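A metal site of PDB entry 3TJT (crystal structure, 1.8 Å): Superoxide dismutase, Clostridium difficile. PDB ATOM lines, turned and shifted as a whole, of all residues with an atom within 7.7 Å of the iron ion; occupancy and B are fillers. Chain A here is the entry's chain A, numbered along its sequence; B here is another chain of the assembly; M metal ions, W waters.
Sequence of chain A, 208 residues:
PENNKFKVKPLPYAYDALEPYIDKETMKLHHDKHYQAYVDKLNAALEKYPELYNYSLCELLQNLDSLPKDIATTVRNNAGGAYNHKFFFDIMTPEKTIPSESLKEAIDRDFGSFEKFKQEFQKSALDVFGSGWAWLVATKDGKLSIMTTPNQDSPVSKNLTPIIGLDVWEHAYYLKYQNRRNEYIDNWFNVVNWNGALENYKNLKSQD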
ATOM      1  N   HIS A  30      19.663  15.236   5.487  1.00  0.00           N
ATOM      2  CA  HIS A  30      20.152  15.977   6.650  1.00  0.00           C
ATOM      3  C   HIS A  30      21.035  17.132   6.192  1.00  0.00           C
ATOM      4  O   HIS A  30      20.896  18.263   6.663  1.00  0.00           O
ATOM      5  CB  HIS A  30      20.917  15.027   7.567  1.00  0.00           C
ATOM      6  CG  HIS A  30      20.969  15.473   9.001  1.00  0.00           C
ATOM      7  ND1 HIS A  30      21.648  14.763   9.959  1.00  0.00           N
ATOM      8  CD2 HIS A  30      20.411  16.530   9.624  1.00  0.00           C
ATOM      9  CE1 HIS A  30      21.519  15.375  11.125  1.00  0.00           C
ATOM     10  NE2 HIS A  30      20.771  16.450  10.947  1.00  0.00           N
ATOM     11  N   HIS A  31      21.934  16.863   5.253  1.00  0.00           N
ATOM     12  CA  HIS A  31      22.845  17.900   4.772  1.00  0.00           C
ATOM     13  C   HIS A  31      22.218  18.808   3.715  1.00  0.00           C
ATOM     14  O   HIS A  31      22.265  20.036   3.824  1.00  0.00           O
ATOM     15  CB  HIS A  31      24.135  17.256   4.208  1.00  0.00           C
ATOM     16  CG  HIS A  31      25.121  18.252   3.684  1.00  0.00           C
ATOM     17  ND1 HIS A  31      25.011  18.850   2.448  1.00  0.00           N
ATOM     18  CD2 HIS A  31      26.256  18.745   4.238  1.00  0.00           C
ATOM     19  CE1 HIS A  31      26.020  19.675   2.268  1.00  0.00           C
ATOM     20  NE2 HIS A  31      26.794  19.625   3.335  1.00  0.00           N
ATOM     21  N   HIS A  34      17.949  19.868   5.408  1.00  0.00           N
ATOM     22  CA  HIS A  34      17.831  20.477   6.738  1.00  0.00           C
ATOM     23  C   HIS A  34      18.917  21.524   6.986  1.00  0.00           C
ATOM     24  O   HIS A  34      18.626  22.669   7.324  1.00  0.00           O
ATOM     25  CB  HIS A  34      17.859  19.425   7.842  1.00  0.00           C
ATOM     26  CG  HIS A  34      16.684  18.489   7.827  1.00  0.00           C
ATOM     27  ND1 HIS A  34      15.482  18.800   8.427  1.00  0.00           N
ATOM     28  CD2 HIS A  34      16.528  17.257   7.288  1.00  0.00           C
ATOM     29  CE1 HIS A  34      14.632  17.796   8.265  1.00  0.00           C
ATOM     30  NE2 HIS A  34      15.245  16.848   7.574  1.00  0.00           N
ATOM     31  N   TYR A  35      20.177  21.129   6.842  1.00  0.00           N
ATOM     32  CA  TYR A  35      21.285  22.067   7.067  1.00  0.00           C
ATOM     33  C   TYR A  35      21.150  23.254   6.116  1.00  0.00           C
ATOM     34  O   TYR A  35      21.209  24.429   6.529  1.00  0.00           O
ATOM     35  CB  TYR A  35      22.608  21.297   6.937  1.00  0.00           C
ATOM     36  CG  TYR A  35      23.890  22.095   7.011  1.00  0.00           C
ATOM     37  CD1 TYR A  35      23.974  23.324   7.674  1.00  0.00           C
ATOM     38  CD2 TYR A  35      25.061  21.579   6.450  1.00  0.00           C
ATOM     39  CE1 TYR A  35      25.180  24.035   7.727  1.00  0.00           C
ATOM     40  CE2 TYR A  35      26.256  22.282   6.498  1.00  0.00           C
ATOM     41  CZ  TYR A  35      26.315  23.503   7.128  1.00  0.00           C
ATOM     42  OH  TYR A  35      27.533  24.146   7.157  1.00  0.00           O
ATOM     43  N   TYR A  38      18.530  25.874   7.300  1.00  0.00           N
ATOM     44  CA  TYR A  38      19.000  26.767   8.371  1.00  0.00           C
ATOM     45  C   TYR A  38      19.847  27.907   7.807  1.00  0.00           C
ATOM     46  O   TYR A  38      19.689  29.059   8.188  1.00  0.00           O
ATOM     47  CB  TYR A  38      19.789  26.012   9.443  1.00  0.00           C
ATOM     48  CG  TYR A  38      18.935  25.045  10.224  1.00  0.00           C
ATOM     49  CD1 TYR A  38      17.809  25.490  10.918  1.00  0.00           C
ATOM     50  CD2 TYR A  38      19.238  23.692  10.268  1.00  0.00           C
ATOM     51  CE1 TYR A  38      17.015  24.598  11.630  1.00  0.00           C
ATOM     52  CE2 TYR A  38      18.455  22.802  10.954  1.00  0.00           C
ATOM     53  CZ  TYR A  38      17.342  23.269  11.648  1.00  0.00           C
ATOM     54  OH  TYR A  38      16.562  22.357  12.341  1.00  0.00           O
ATOM     55  N   GLY A  81      21.100  26.190  14.010  1.00  0.00           N
ATOM     56  CA  GLY A  81      21.006  25.057  13.092  1.00  0.00           C
ATOM     57  C   GLY A  81      22.235  24.968  12.203  1.00  0.00           C
ATOM     58  O   GLY A  81      22.798  23.897  12.006  1.00  0.00           O
ATOM     59  N   ASN A  84      25.407  24.058  14.403  1.00  0.00           N
ATOM     60  CA  ASN A  84      25.343  22.705  14.944  1.00  0.00           C
ATOM     61  C   ASN A  84      25.558  21.646  13.856  1.00  0.00           C
ATOM     62  O   ASN A  84      26.225  20.637  14.092  1.00  0.00           O
ATOM     63  CB  ASN A  84      24.010  22.450  15.657  1.00  0.00           C
ATOM     64  CG  ASN A  84      23.865  23.240  16.954  1.00  0.00           C
ATOM     65  OD1 ASN A  84      24.843  23.764  17.503  1.00  0.00           O
ATOM     66  ND2 ASN A  84      22.632  23.339  17.463  1.00  0.00           N
ATOM     67  N   HIS A  85      24.997  21.859  12.672  1.00  0.00           N
ATOM     68  CA  HIS A  85      25.120  20.867  11.622  1.00  0.00           C
ATOM     69  C   HIS A  85      26.517  20.857  11.017  1.00  0.00           C
ATOM     70  O   HIS A  85      27.064  19.789  10.746  1.00  0.00           O
ATOM     71  CB  HIS A  85      24.024  21.038  10.572  1.00  0.00           C
ATOM     72  CG  HIS A  85      22.695  20.558  11.054  1.00  0.00           C
ATOM     73  ND1 HIS A  85      21.863  21.346  11.829  1.00  0.00           N
ATOM     74  CD2 HIS A  85      22.093  19.352  10.961  1.00  0.00           C
ATOM     75  CE1 HIS A  85      20.781  20.652  12.152  1.00  0.00           C
ATOM     76  NE2 HIS A  85      20.910  19.438  11.648  1.00  0.00           N
ATOM     77  N   PHE A  88      28.417  18.972  13.502  1.00  0.00           N
ATOM     78  CA  PHE A  88      28.035  17.564  13.522  1.00  0.00           C
ATOM     79  C   PHE A  88      28.652  16.770  12.353  1.00  0.00           C
ATOM     80  O   PHE A  88      29.197  15.679  12.558  1.00  0.00           O
ATOM     81  CB  PHE A  88      26.512  17.457  13.500  1.00  0.00           C
ATOM     82  CG  PHE A  88      25.980  16.054  13.622  1.00  0.00           C
ATOM     83  CD1 PHE A  88      26.317  15.266  14.708  1.00  0.00           C
ATOM     84  CD2 PHE A  88      25.126  15.542  12.650  1.00  0.00           C
ATOM     85  CE1 PHE A  88      25.816  13.965  14.829  1.00  0.00           C
ATOM     86  CE2 PHE A  88      24.622  14.238  12.762  1.00  0.00           C
ATOM     87  CZ  PHE A  88      24.961  13.453  13.857  1.00  0.00           C
ATOM     88  N   PHE A  89      28.547  17.292  11.142  1.00  0.00           N
ATOM     89  CA  PHE A  89      29.115  16.556  10.012  1.00  0.00           C
ATOM     90  C   PHE A  89      30.646  16.494  10.137  1.00  0.00           C
ATOM     91  O   PHE A  89      31.251  15.493   9.758  1.00  0.00           O
ATOM     92  CB  PHE A  89      28.644  17.126   8.681  1.00  0.00           C
ATOM     93  CG  PHE A  89      27.139  17.042   8.500  1.00  0.00           C
ATOM     94  CD1 PHE A  89      26.466  15.854   8.746  1.00  0.00           C
ATOM     95  CD2 PHE A  89      26.408  18.152   8.104  1.00  0.00           C
ATOM     96  CE1 PHE A  89      25.082  15.769   8.604  1.00  0.00           C
ATOM     97  CE2 PHE A  89      25.024  18.076   7.947  1.00  0.00           C
ATOM     98  CZ  PHE A  89      24.366  16.888   8.199  1.00  0.00           C
ATOM     99  N   GLY A 132      16.578  17.845  20.030  1.00  0.00           N
ATOM    100  CA  GLY A 132      17.745  18.476  20.646  1.00  0.00           C
ATOM    101  C   GLY A 132      19.029  17.734  20.397  1.00  0.00           C
ATOM    102  O   GLY A 132      19.125  16.945  19.461  1.00  0.00           O
ATOM    103  N   TRP A 133      20.025  18.006  21.243  1.00  0.00           N
ATOM    104  CA  TRP A 133      21.412  17.564  21.052  1.00  0.00           C
ATOM    105  C   TRP A 133      22.001  17.116  22.378  1.00  0.00           C
ATOM    106  O   TRP A 133      21.652  17.655  23.431  1.00  0.00           O
ATOM    107  CB  TRP A 133      22.252  18.730  20.525  1.00  0.00           C
ATOM    108  CG  TRP A 133      21.906  19.182  19.163  1.00  0.00           C
ATOM    109  CD1 TRP A 133      20.838  19.954  18.799  1.00  0.00           C
ATOM    110  CD2 TRP A 133      22.623  18.899  17.955  1.00  0.00           C
ATOM    111  NE1 TRP A 133      20.842  20.164  17.443  1.00  0.00           N
ATOM    112  CE2 TRP A 133      21.927  19.524  16.899  1.00  0.00           C
ATOM    113  CE3 TRP A 133      23.788  18.194  17.664  1.00  0.00           C
ATOM    114  CZ2 TRP A 133      22.352  19.456  15.575  1.00  0.00           C
ATOM    115  CZ3 TRP A 133      24.226  18.122  16.336  1.00  0.00           C
ATOM    116  CH2 TRP A 133      23.510  18.752  15.319  1.00  0.00           C
ATOM    117  N   ASN A 151      16.192  21.772  20.763  1.00  0.00           N
ATOM    118  CA  ASN A 151      16.038  22.378  19.450  1.00  0.00           C
ATOM    119  C   ASN A 151      17.402  22.663  18.804  1.00  0.00           C
ATOM    120  O   ASN A 151      18.178  21.736  18.664  1.00  0.00           O
ATOM    121  CB  ASN A 151      15.110  23.594  19.535  1.00  0.00           C
ATOM    122  CG  ASN A 151      13.768  23.210  20.142  1.00  0.00           C
ATOM    123  OD1 ASN A 151      13.246  22.141  19.841  1.00  0.00           O
ATOM    124  ND2 ASN A 151      13.228  24.067  21.020  1.00  0.00           N
ATOM    125  N   GLN A 152      17.685  23.904  18.421  1.00  0.00           N
ATOM    126  CA  GLN A 152      19.033  24.198  17.899  1.00  0.00           C
ATOM    127  C   GLN A 152      19.837  25.100  18.825  1.00  0.00           C
ATOM    128  O   GLN A 152      20.760  25.782  18.379  1.00  0.00           O
ATOM    129  CB  GLN A 152      19.013  24.790  16.492  1.00  0.00           C
ATOM    130  CG  GLN A 152      18.327  23.904  15.423  1.00  0.00           C
ATOM    131  CD  GLN A 152      19.043  22.577  15.179  1.00  0.00           C
ATOM    132  OE1 GLN A 152      20.212  22.387  15.580  1.00  0.00           O
ATOM    133  NE2 GLN A 152      18.361  21.662  14.519  1.00  0.00           N
ATOM    134  N   ASP A 167      23.238  14.826  17.266  1.00  0.00           N
ATOM    135  CA  ASP A 167      21.916  15.291  16.884  1.00  0.00           C
ATOM    136  C   ASP A 167      20.897  14.207  17.205  1.00  0.00           C
ATOM    137  O   ASP A 167      20.970  13.108  16.666  1.00  0.00           O
ATOM    138  CB  ASP A 167      21.936  15.584  15.382  1.00  0.00           C
ATOM    139  CG  ASP A 167      20.676  16.272  14.876  1.00  0.00           C
ATOM    140  OD1 ASP A 167      19.704  16.422  15.649  1.00  0.00           O
ATOM    141  OD2 ASP A 167      20.673  16.683  13.695  1.00  0.00           O
ATOM    142  N   VAL A 168      19.945  14.494  18.088  1.00  0.00           N
ATOM    143  CA  VAL A 168      18.873  13.523  18.353  1.00  0.00           C
ATOM    144  C   VAL A 168      17.489  14.019  17.957  1.00  0.00           C
ATOM    145  O   VAL A 168      16.474  13.502  18.450  1.00  0.00           O
ATOM    146  CB  VAL A 168      18.871  12.963  19.823  1.00  0.00           C
ATOM    147  CG1 VAL A 168      20.114  12.105  20.072  1.00  0.00           C
ATOM    148  CG2 VAL A 168      18.775  14.088  20.849  1.00  0.00           C
ATOM    149  N   TRP A 169      17.437  15.006  17.073  1.00  0.00           N
ATOM    150  CA  TRP A 169      16.193  15.315  16.365  1.00  0.00           C
ATOM    151  C   TRP A 169      15.808  14.029  15.643  1.00  0.00           C
ATOM    152  O   TRP A 169      16.685  13.285  15.192  1.00  0.00           O
ATOM    153  CB  TRP A 169      16.403  16.408  15.325  1.00  0.00           C
ATOM    154  CG  TRP A 169      16.483  17.818  15.858  1.00  0.00           C
ATOM    155  CD1 TRP A 169      17.357  18.301  16.790  1.00  0.00           C
ATOM    156  CD2 TRP A 169      15.654  18.914  15.454  1.00  0.00           C
ATOM    157  NE1 TRP A 169      17.116  19.649  17.005  1.00  0.00           N
ATOM    158  CE2 TRP A 169      16.095  20.047  16.192  1.00  0.00           C
ATOM    159  CE3 TRP A 169      14.608  19.067  14.550  1.00  0.00           C
ATOM    160  CZ2 TRP A 169      15.499  21.306  16.043  1.00  0.00           C
ATOM    161  CZ3 TRP A 169      14.017  20.327  14.388  1.00  0.00           C
ATOM    162  CH2 TRP A 169      14.465  21.430  15.134  1.00  0.00           C
ATOM    163  N   GLU A 170      14.513  13.786  15.506  1.00  0.00           N
ATOM    164  CA  GLU A 170      14.101  12.564  14.846  1.00  0.00           C
ATOM    165  C   GLU A 170      14.527  12.485  13.369  1.00  0.00           C
ATOM    166  O   GLU A 170      14.742  11.394  12.848  1.00  0.00           O
ATOM    167  CB  GLU A 170      12.593  12.321  15.045  1.00  0.00           C
ATOM    168  CG  GLU A 170      12.294  11.878  16.480  1.00  0.00           C
ATOM    169  CD  GLU A 170      10.805  11.872  16.821  1.00  0.00           C
ATOM    170  OE1 GLU A 170      10.049  12.706  16.277  1.00  0.00           O
ATOM    171  OE2 GLU A 170      10.424  11.019  17.641  1.00  0.00           O
ATOM    172  N   HIS A 171      14.677  13.634  12.706  1.00  0.00           N
ATOM    173  CA  HIS A 171      15.135  13.576  11.312  1.00  0.00           C
ATOM    174  C   HIS A 171      16.505  12.907  11.186  1.00  0.00           C
ATOM    175  O   HIS A 171      16.868  12.398  10.118  1.00  0.00           O
ATOM    176  CB  HIS A 171      15.087  14.923  10.575  1.00  0.00           C
ATOM    177  CG  HIS A 171      15.983  15.983  11.147  1.00  0.00           C
ATOM    178  ND1 HIS A 171      15.498  17.183  11.628  1.00  0.00           N
ATOM    179  CD2 HIS A 171      17.329  16.035  11.302  1.00  0.00           C
ATOM    180  CE1 HIS A 171      16.515  17.928  12.052  1.00  0.00           C
ATOM    181  NE2 HIS A 171      17.627  17.243  11.871  1.00  0.00           N
ATOM    182  N   ALA A 172      17.266  12.901  12.274  1.00  0.00           N
ATOM    183  CA  ALA A 172      18.634  12.383  12.206  1.00  0.00           C
ATOM    184  C   ALA A 172      18.692  10.869  12.211  1.00  0.00           C
ATOM    185  O   ALA A 172      19.734  10.294  11.869  1.00  0.00           O
ATOM    186  CB  ALA A 172      19.480  12.940  13.353  1.00  0.00           C
ATOM    187  N   TYR A 184      20.511   3.990  17.445  1.00  0.00           N
ATOM    188  CA  TYR A 184      21.176   5.076  16.738  1.00  0.00           C
ATOM    189  C   TYR A 184      22.342   5.606  17.557  1.00  0.00           C
ATOM    190  O   TYR A 184      23.449   5.787  17.055  1.00  0.00           O
ATOM    191  CB  TYR A 184      20.177   6.191  16.460  1.00  0.00           C
ATOM    192  CG  TYR A 184      20.760   7.531  16.032  1.00  0.00           C
ATOM    193  CD1 TYR A 184      21.468   7.676  14.850  1.00  0.00           C
ATOM    194  CD2 TYR A 184      20.530   8.664  16.810  1.00  0.00           C
ATOM    195  CE1 TYR A 184      21.962   8.929  14.449  1.00  0.00           C
ATOM    196  CE2 TYR A 184      21.016   9.903  16.428  1.00  0.00           C
ATOM    197  CZ  TYR A 184      21.725  10.038  15.260  1.00  0.00           C
ATOM    198  OH  TYR A 184      22.180  11.283  14.897  1.00  0.00           O
ATOM    199  N   GLU B 170       8.623  15.025  14.193  1.00  0.00           N
ATOM    200  CA  GLU B 170       9.071  14.390  12.965  1.00  0.00           C
ATOM    201  C   GLU B 170       8.672  12.916  12.858  1.00  0.00           C
ATOM    202  O   GLU B 170       8.483  12.409  11.747  1.00  0.00           O
ATOM    203  CB  GLU B 170      10.581  14.620  12.758  1.00  0.00           C
ATOM    204  CG  GLU B 170      10.853  16.065  12.349  1.00  0.00           C
ATOM    205  CD  GLU B 170      12.343  16.439  12.375  1.00  0.00           C
ATOM    206  OE1 GLU B 170      13.091  15.895  13.207  1.00  0.00           O
ATOM    207  OE2 GLU B 170      12.727  17.281  11.547  1.00  0.00           O
HETATM  208 FE    FE M   1      19.723  17.690  12.363  1.00  0.00          FE
HETATM  209  O   HOH W   1      18.966  18.845  14.126  1.00  0.00           O
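The iron ion is bound by the side-chain carboxylate (OD2) of Asp 167 (1.9 Å), a ring nitrogen (NE2) of His 30 (2.2 Å), a ring nitrogen (NE2) of His 171 (2.2 Å), a ring nitrogen (NE2) of His 85 (2.2 Å) and water W1 (2.2 Å).
Four residues have an atom within 4 Å of the iron ion: His 30, His 85, Asp 167 and His 171.
The nearest printed residue that does not touch the iron ion is Trp 133 (4.5 Å).
Water W1 bridges the side-chain amide nitrogen (NE2) of Gln 152 and the side-chain carboxylate (OD1) of Asp 167.
OH of Tyr 184 lies within hydrogen-bond range of O of Asp 167, at 2.8 Å.
O of His 30 is in hydrogen-bond range of N of Tyr 35 (3.0 Å).
A ring nitrogen (ND1) of His 85 sits at hydrogen-bond distance from the backbone carbonyl oxygen (O) of Gly 81, at 2.7 Å.
A ring nitrogen (ND1) of His 171 is in hydrogen-bond range of the side-chain carboxylate (OE2) of Glu 170 of chain B (2.8 Å).
The side-chain carboxylate (OD1) of Asp 167 sits at hydrogen-bond distance from the backbone NH (N) of Trp 169 (3.0 Å).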
